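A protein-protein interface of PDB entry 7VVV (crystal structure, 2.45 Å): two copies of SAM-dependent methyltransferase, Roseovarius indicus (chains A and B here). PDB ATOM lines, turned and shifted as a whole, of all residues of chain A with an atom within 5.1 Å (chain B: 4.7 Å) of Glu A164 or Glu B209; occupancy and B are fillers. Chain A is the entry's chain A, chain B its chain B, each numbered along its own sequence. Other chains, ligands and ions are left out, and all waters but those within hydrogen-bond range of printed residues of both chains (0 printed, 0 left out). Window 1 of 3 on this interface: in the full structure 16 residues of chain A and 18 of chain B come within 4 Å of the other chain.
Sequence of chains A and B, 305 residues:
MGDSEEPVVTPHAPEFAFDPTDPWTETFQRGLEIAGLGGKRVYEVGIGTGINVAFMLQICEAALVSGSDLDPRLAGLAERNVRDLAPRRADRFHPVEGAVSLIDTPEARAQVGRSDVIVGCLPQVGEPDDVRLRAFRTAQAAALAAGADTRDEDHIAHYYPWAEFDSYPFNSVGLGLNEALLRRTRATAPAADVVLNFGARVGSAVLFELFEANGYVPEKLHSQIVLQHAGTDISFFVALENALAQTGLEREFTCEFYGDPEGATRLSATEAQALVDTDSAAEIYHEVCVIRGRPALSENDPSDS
Among the printed residues, merely in contact across the chains: Glu A164 with Glu B209, Tyr A168 with Ala B213, Glu A164 with Ala B205, Phe A165 with Glu B209 and Ser A167 with Phe B170.
OH of Tyr A168 sits at hydrogen-bond distance from OE2 of Glu B209, 2.4 Å away. The side-chain carboxylate (OE2) of Glu B209 is in salt-bridge range of the guanidinium group (NH1) of Arg A184. NE of Arg A184 is in salt-bridge range of OE1 of Glu B212 (3.8 Å).
No position is printed for both chains.
The guanidinium group of Arg A184 sits close to the backbone carbonyl oxygen of Ala A180, at 3.2 Å.
Printed residues of chain B that touch a printed residue of chain A: Phe B170, Ala B205, Glu B209, Glu B212 and Ala B213. Hydrophobic or aromatic side chains of chain B that line the printed part of chain A: Phe B170, Ala B205 and Ala B213. Of the 10 printed residues of chain A, 5 touch a printed residue of chain B. Hydrophobic or aromatic side chains of chain A that line the printed part of chain B: Phe A165 and Tyr A168. Among the printed residues, Asp or Glu carboxylates within 4 Å of a Lys or Arg side-chain nitrogen of the other chain: Arg A184 with Glu B209 (3.2 Å) and Arg A184 with Glu B212 (3.8 Å).
Of the printed residues of chain B, Glu A164 touches Ala B205 and Glu B209. Of chain A, only Glu A164, Phe A165, Tyr A168 and Arg A184 come within 4 Å of Glu B209. Printed residues of chain A within 4 Å of Ala B213: Tyr A168. Printed residues of chain B within 4 Å of Phe A165: Glu B209 (3.7 Å). Of the printed residues of chain B, Tyr A168 touches Glu B209 (2.4 Å) and Ala B213 (3.1 Å). Of the printed residues of chain B, Arg A184 touches Glu B209 and Glu B212. Printed residues of chain A within 4 Å of Glu B212: Arg A184. Leu B210 touches none of the printed residues of chain A. Ala A163 touches none of the printed residues of chain B. The nearest printed residue of chain A that does not touch Glu B212 is Tyr A168 (4.6 Å).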
ATOM      1  N   PRO A 161      -7.844 -35.739 -28.187  1.00  0.00           N
ATOM      2  CA  PRO A 161      -7.695 -35.232 -26.825  1.00  0.00           C
ATOM      3  C   PRO A 161      -8.963 -35.579 -26.089  1.00  0.00           C
ATOM      4  O   PRO A 161      -9.877 -36.129 -26.654  1.00  0.00           O
ATOM      5  CB  PRO A 161      -7.637 -33.738 -27.006  1.00  0.00           C
ATOM      6  CG  PRO A 161      -8.553 -33.499 -28.130  1.00  0.00           C
ATOM      7  CD  PRO A 161      -8.145 -34.545 -29.090  1.00  0.00           C
ATOM      8  N   TRP A 162      -9.026 -35.186 -24.846  1.00  0.00           N
ATOM      9  CA  TRP A 162     -10.139 -35.559 -24.056  1.00  0.00           C
ATOM     10  C   TRP A 162     -10.629 -34.542 -23.065  1.00  0.00           C
ATOM     11  O   TRP A 162     -11.725 -34.619 -22.668  1.00  0.00           O
ATOM     12  CB  TRP A 162      -9.695 -36.784 -23.279  1.00  0.00           C
ATOM     13  CG  TRP A 162      -8.564 -36.413 -22.478  1.00  0.00           C
ATOM     14  CD1 TRP A 162      -7.322 -36.155 -22.923  1.00  0.00           C
ATOM     15  CD2 TRP A 162      -8.584 -36.076 -21.115  1.00  0.00           C
ATOM     16  NE1 TRP A 162      -6.548 -35.738 -21.910  1.00  0.00           N
ATOM     17  CE2 TRP A 162      -7.306 -35.672 -20.777  1.00  0.00           C
ATOM     18  CE3 TRP A 162      -9.554 -36.100 -20.139  1.00  0.00           C
ATOM     19  CZ2 TRP A 162      -6.968 -35.302 -19.492  1.00  0.00           C
ATOM     20  CZ3 TRP A 162      -9.219 -35.735 -18.871  1.00  0.00           C
ATOM     21  CH2 TRP A 162      -7.940 -35.342 -18.553  1.00  0.00           C
ATOM     22  N   ALA A 163      -9.821 -33.620 -22.639  1.00  0.00           N
ATOM     23  CA  ALA A 163     -10.255 -32.679 -21.650  1.00  0.00           C
ATOM     24  C   ALA A 163     -11.381 -31.750 -22.011  1.00  0.00           C
ATOM     25  O   ALA A 163     -12.156 -31.422 -21.197  1.00  0.00           O
ATOM     26  CB  ALA A 163      -9.084 -31.938 -21.083  1.00  0.00           C
ATOM     27  N   GLU A 164     -11.472 -31.316 -23.230  1.00  0.00           N
ATOM     28  CA  GLU A 164     -12.570 -30.410 -23.565  1.00  0.00           C
ATOM     29  C   GLU A 164     -13.903 -31.134 -23.690  1.00  0.00           C
ATOM     30  O   GLU A 164     -14.949 -30.469 -23.701  1.00  0.00           O
ATOM     31  CB  GLU A 164     -12.269 -29.630 -24.856  1.00  0.00           C
ATOM     32  CG  GLU A 164     -12.143 -30.484 -26.107  1.00  0.00           C
ATOM     33  CD  GLU A 164     -10.698 -30.737 -26.475  1.00  0.00           C
ATOM     34  OE1 GLU A 164     -10.323 -30.523 -27.656  1.00  0.00           O
ATOM     35  OE2 GLU A 164      -9.938 -31.138 -25.567  1.00  0.00           O
ATOM     36  N   PHE A 165     -13.905 -32.465 -23.759  1.00  0.00           N
ATOM     37  CA  PHE A 165     -15.151 -33.218 -23.799  1.00  0.00           C
ATOM     38  C   PHE A 165     -15.538 -33.763 -22.439  1.00  0.00           C
ATOM     39  O   PHE A 165     -16.508 -34.517 -22.335  1.00  0.00           O
ATOM     40  CB  PHE A 165     -15.061 -34.337 -24.833  1.00  0.00           C
ATOM     41  CG  PHE A 165     -14.473 -33.880 -26.131  1.00  0.00           C
ATOM     42  CD1 PHE A 165     -15.127 -32.925 -26.907  1.00  0.00           C
ATOM     43  CD2 PHE A 165     -13.228 -34.326 -26.548  1.00  0.00           C
ATOM     44  CE1 PHE A 165     -14.575 -32.466 -28.108  1.00  0.00           C
ATOM     45  CE2 PHE A 165     -12.668 -33.853 -27.752  1.00  0.00           C
ATOM     46  CZ  PHE A 165     -13.344 -32.933 -28.526  1.00  0.00           C
ATOM     47  N   ASP A 166     -14.845 -33.341 -21.387  1.00  0.00           N
ATOM     48  CA  ASP A 166     -15.031 -33.941 -20.074  1.00  0.00           C
ATOM     49  C   ASP A 166     -16.307 -33.462 -19.401  1.00  0.00           C
ATOM     50  O   ASP A 166     -16.889 -34.195 -18.596  1.00  0.00           O
ATOM     51  CB  ASP A 166     -13.811 -33.631 -19.194  1.00  0.00           C
ATOM     52  CG  ASP A 166     -13.841 -34.359 -17.851  1.00  0.00           C
ATOM     53  OD1 ASP A 166     -13.824 -35.609 -17.848  1.00  0.00           O
ATOM     54  OD2 ASP A 166     -13.853 -33.681 -16.796  1.00  0.00           O
ATOM     55  N   SER A 167     -16.743 -32.241 -19.694  1.00  0.00           N
ATOM     56  CA  SER A 167     -17.864 -31.650 -18.988  1.00  0.00           C
ATOM     57  C   SER A 167     -19.202 -32.139 -19.518  1.00  0.00           C
ATOM     58  O   SER A 167     -20.225 -31.911 -18.860  1.00  0.00           O
ATOM     59  CB  SER A 167     -17.802 -30.114 -19.086  1.00  0.00           C
ATOM     60  OG  SER A 167     -18.362 -29.620 -20.304  1.00  0.00           O
ATOM     61  N   TYR A 168     -19.205 -32.787 -20.681  1.00  0.00           N
ATOM     62  CA  TYR A 168     -20.433 -33.231 -21.312  1.00  0.00           C
ATOM     63  C   TYR A 168     -21.231 -34.138 -20.379  1.00  0.00           C
ATOM     64  O   TYR A 168     -20.659 -35.034 -19.742  1.00  0.00           O
ATOM     65  CB  TYR A 168     -20.126 -33.962 -22.617  1.00  0.00           C
ATOM     66  CG  TYR A 168     -19.913 -33.011 -23.754  1.00  0.00           C
ATOM     67  CD1 TYR A 168     -20.989 -32.531 -24.488  1.00  0.00           C
ATOM     68  CD2 TYR A 168     -18.636 -32.563 -24.090  1.00  0.00           C
ATOM     69  CE1 TYR A 168     -20.807 -31.618 -25.538  1.00  0.00           C
ATOM     70  CE2 TYR A 168     -18.437 -31.667 -25.148  1.00  0.00           C
ATOM     71  CZ  TYR A 168     -19.539 -31.195 -25.861  1.00  0.00           C
ATOM     72  OH  TYR A 168     -19.376 -30.310 -26.901  1.00  0.00           O
ATOM     73  N   ALA A 180     -20.607 -34.663 -28.098  1.00  0.00           N
ATOM     74  CA  ALA A 180     -20.068 -33.515 -28.726  1.00  0.00           C
ATOM     75  C   ALA A 180     -20.196 -33.498 -30.205  1.00  0.00           C
ATOM     76  O   ALA A 180     -20.252 -32.470 -30.757  1.00  0.00           O
ATOM     77  CB  ALA A 180     -18.645 -33.311 -28.312  1.00  0.00           C
ATOM     78  N   ARG A 184     -22.587 -30.878 -32.740  1.00  0.00           N
ATOM     79  CA  ARG A 184     -22.152 -30.339 -33.971  1.00  0.00           C
ATOM     80  C   ARG A 184     -23.043 -30.640 -35.121  1.00  0.00           C
ATOM     81  O   ARG A 184     -23.364 -29.778 -35.845  1.00  0.00           O
ATOM     82  CB  ARG A 184     -20.749 -30.768 -34.278  1.00  0.00           C
ATOM     83  CG  ARG A 184     -19.705 -30.039 -33.514  1.00  0.00           C
ATOM     84  CD  ARG A 184     -18.657 -31.006 -33.100  1.00  0.00           C
ATOM     85  NE  ARG A 184     -17.429 -30.429 -32.659  1.00  0.00           N
ATOM     86  CZ  ARG A 184     -17.162 -30.070 -31.438  1.00  0.00           C
ATOM     87  NH1 ARG A 184     -18.045 -30.146 -30.520  1.00  0.00           N
ATOM     88  NH2 ARG A 184     -16.013 -29.586 -31.165  1.00  0.00           N
ATOM     89  N   PHE B 170     -20.459 -26.460 -18.451  1.00  0.00           N
ATOM     90  CA  PHE B 170     -19.243 -25.669 -18.514  1.00  0.00           C
ATOM     91  C   PHE B 170     -19.008 -24.835 -17.273  1.00  0.00           C
ATOM     92  O   PHE B 170     -18.019 -24.096 -17.230  1.00  0.00           O
ATOM     93  CB  PHE B 170     -19.240 -24.809 -19.778  1.00  0.00           C
ATOM     94  CG  PHE B 170     -18.761 -25.563 -20.973  1.00  0.00           C
ATOM     95  CD1 PHE B 170     -17.400 -25.665 -21.242  1.00  0.00           C
ATOM     96  CD2 PHE B 170     -19.663 -26.251 -21.779  1.00  0.00           C
ATOM     97  CE1 PHE B 170     -16.941 -26.402 -22.333  1.00  0.00           C
ATOM     98  CE2 PHE B 170     -19.218 -26.992 -22.866  1.00  0.00           C
ATOM     99  CZ  PHE B 170     -17.850 -27.074 -23.141  1.00  0.00           C
ATOM    100  N   ALA B 205      -8.842 -24.876 -26.130  1.00  0.00           N
ATOM    101  CA  ALA B 205      -9.658 -26.017 -26.540  1.00  0.00           C
ATOM    102  C   ALA B 205     -10.974 -26.037 -25.776  1.00  0.00           C
ATOM    103  O   ALA B 205     -12.029 -26.331 -26.346  1.00  0.00           O
ATOM    104  CB  ALA B 205      -8.897 -27.325 -26.326  1.00  0.00           C
ATOM    105  N   VAL B 206     -10.929 -25.709 -24.481  1.00  0.00           N
ATOM    106  CA  VAL B 206     -12.129 -25.692 -23.650  1.00  0.00           C
ATOM    107  C   VAL B 206     -13.026 -24.514 -24.028  1.00  0.00           C
ATOM    108  O   VAL B 206     -14.244 -24.671 -24.190  1.00  0.00           O
ATOM    109  CB  VAL B 206     -11.733 -25.650 -22.160  1.00  0.00           C
ATOM    110  CG1 VAL B 206     -12.909 -25.271 -21.288  1.00  0.00           C
ATOM    111  CG2 VAL B 206     -11.203 -26.981 -21.732  1.00  0.00           C
ATOM    112  N   LEU B 207     -12.435 -23.317 -24.174  1.00  0.00           N
ATOM    113  CA  LEU B 207     -13.215 -22.141 -24.566  1.00  0.00           C
ATOM    114  C   LEU B 207     -13.896 -22.362 -25.908  1.00  0.00           C
ATOM    115  O   LEU B 207     -15.059 -21.984 -26.090  1.00  0.00           O
ATOM    116  CB  LEU B 207     -12.331 -20.892 -24.635  1.00  0.00           C
ATOM    117  CG  LEU B 207     -11.597 -20.444 -23.366  1.00  0.00           C
ATOM    118  CD1 LEU B 207     -10.707 -19.261 -23.660  1.00  0.00           C
ATOM    119  CD2 LEU B 207     -12.548 -20.143 -22.198  1.00  0.00           C
ATOM    120  N   PHE B 208     -13.229 -22.993 -26.812  1.00  0.00           N
ATOM    121  CA  PHE B 208     -13.819 -23.214 -28.047  1.00  0.00           C
ATOM    122  C   PHE B 208     -14.900 -24.228 -27.905  1.00  0.00           C
ATOM    123  O   PHE B 208     -15.831 -24.195 -28.628  1.00  0.00           O
ATOM    124  CB  PHE B 208     -12.797 -23.680 -29.039  1.00  0.00           C
ATOM    125  CG  PHE B 208     -12.108 -22.595 -29.747  1.00  0.00           C
ATOM    126  CD1 PHE B 208     -11.822 -21.453 -29.127  1.00  0.00           C
ATOM    127  CD2 PHE B 208     -11.751 -22.742 -31.041  1.00  0.00           C
ATOM    128  CE1 PHE B 208     -11.209 -20.452 -29.785  1.00  0.00           C
ATOM    129  CE2 PHE B 208     -11.128 -21.752 -31.706  1.00  0.00           C
ATOM    130  CZ  PHE B 208     -10.851 -20.607 -31.072  1.00  0.00           C
ATOM    131  N   GLU B 209     -14.743 -25.137 -26.949  1.00  0.00           N
ATOM    132  CA  GLU B 209     -15.728 -26.185 -26.713  1.00  0.00           C
ATOM    133  C   GLU B 209     -17.049 -25.609 -26.218  1.00  0.00           C
ATOM    134  O   GLU B 209     -18.120 -26.118 -26.549  1.00  0.00           O
ATOM    135  CB  GLU B 209     -15.192 -27.209 -25.711  1.00  0.00           C
ATOM    136  CG  GLU B 209     -15.841 -28.579 -25.814  1.00  0.00           C
ATOM    137  CD  GLU B 209     -16.056 -29.015 -27.250  1.00  0.00           C
ATOM    138  OE1 GLU B 209     -15.152 -28.791 -28.082  1.00  0.00           O
ATOM    139  OE2 GLU B 209     -17.129 -29.581 -27.547  1.00  0.00           O
ATOM    140  N   LEU B 210     -16.969 -24.548 -25.421  1.00  0.00           N
ATOM    141  CA  LEU B 210     -18.136 -23.932 -24.898  1.00  0.00           C
ATOM    142  C   LEU B 210     -18.989 -23.423 -26.039  1.00  0.00           C
ATOM    143  O   LEU B 210     -20.143 -23.487 -25.986  1.00  0.00           O
ATOM    144  CB  LEU B 210     -17.761 -22.830 -23.957  1.00  0.00           C
ATOM    145  CG  LEU B 210     -18.722 -21.731 -23.631  1.00  0.00           C
ATOM    146  CD1 LEU B 210     -19.675 -22.110 -22.561  1.00  0.00           C
ATOM    147  CD2 LEU B 210     -17.977 -20.520 -23.220  1.00  0.00           C
ATOM    148  N   PHE B 211     -18.406 -22.932 -27.090  1.00  0.00           N
ATOM    149  CA  PHE B 211     -19.224 -22.520 -28.233  1.00  0.00           C
ATOM    150  C   PHE B 211     -19.687 -23.722 -29.046  1.00  0.00           C
ATOM    151  O   PHE B 211     -20.863 -23.828 -29.400  1.00  0.00           O
ATOM    152  CB  PHE B 211     -18.449 -21.548 -29.142  1.00  0.00           C
ATOM    153  CG  PHE B 211     -18.236 -20.197 -28.536  1.00  0.00           C
ATOM    154  CD1 PHE B 211     -17.142 -19.956 -27.723  1.00  0.00           C
ATOM    155  CD2 PHE B 211     -19.132 -19.163 -28.775  1.00  0.00           C
ATOM    156  CE1 PHE B 211     -16.941 -18.702 -27.162  1.00  0.00           C
ATOM    157  CE2 PHE B 211     -18.951 -17.928 -28.207  1.00  0.00           C
ATOM    158  CZ  PHE B 211     -17.851 -17.688 -27.404  1.00  0.00           C
ATOM    159  N   GLU B 212     -18.766 -24.623 -29.376  1.00  0.00           N
ATOM    160  CA  GLU B 212     -19.116 -25.769 -30.203  1.00  0.00           C
ATOM    161  C   GLU B 212     -20.213 -26.608 -29.553  1.00  0.00           C
ATOM    162  O   GLU B 212     -21.096 -27.121 -30.241  1.00  0.00           O
ATOM    163  CB  GLU B 212     -17.866 -26.615 -30.458  1.00  0.00           C
ATOM    164  CG  GLU B 212     -16.853 -25.963 -31.410  1.00  0.00           C
ATOM    165  CD  GLU B 212     -17.241 -26.177 -32.865  1.00  0.00           C
ATOM    166  OE1 GLU B 212     -18.327 -26.727 -33.116  1.00  0.00           O
ATOM    167  OE2 GLU B 212     -16.451 -25.834 -33.767  1.00  0.00           O
ATOM    168  N   ALA B 213     -20.178 -26.753 -28.227  1.00  0.00           N
ATOM    169  CA  ALA B 213     -21.213 -27.510 -27.541  1.00  0.00           C
ATOM    170  C   ALA B 213     -22.582 -26.849 -27.669  1.00  0.00           C
ATOM    171  O   ALA B 213     -23.602 -27.512 -27.433  1.00  0.00           O
ATOM    172  CB  ALA B 213     -20.865 -27.669 -26.060  1.00  0.00           C
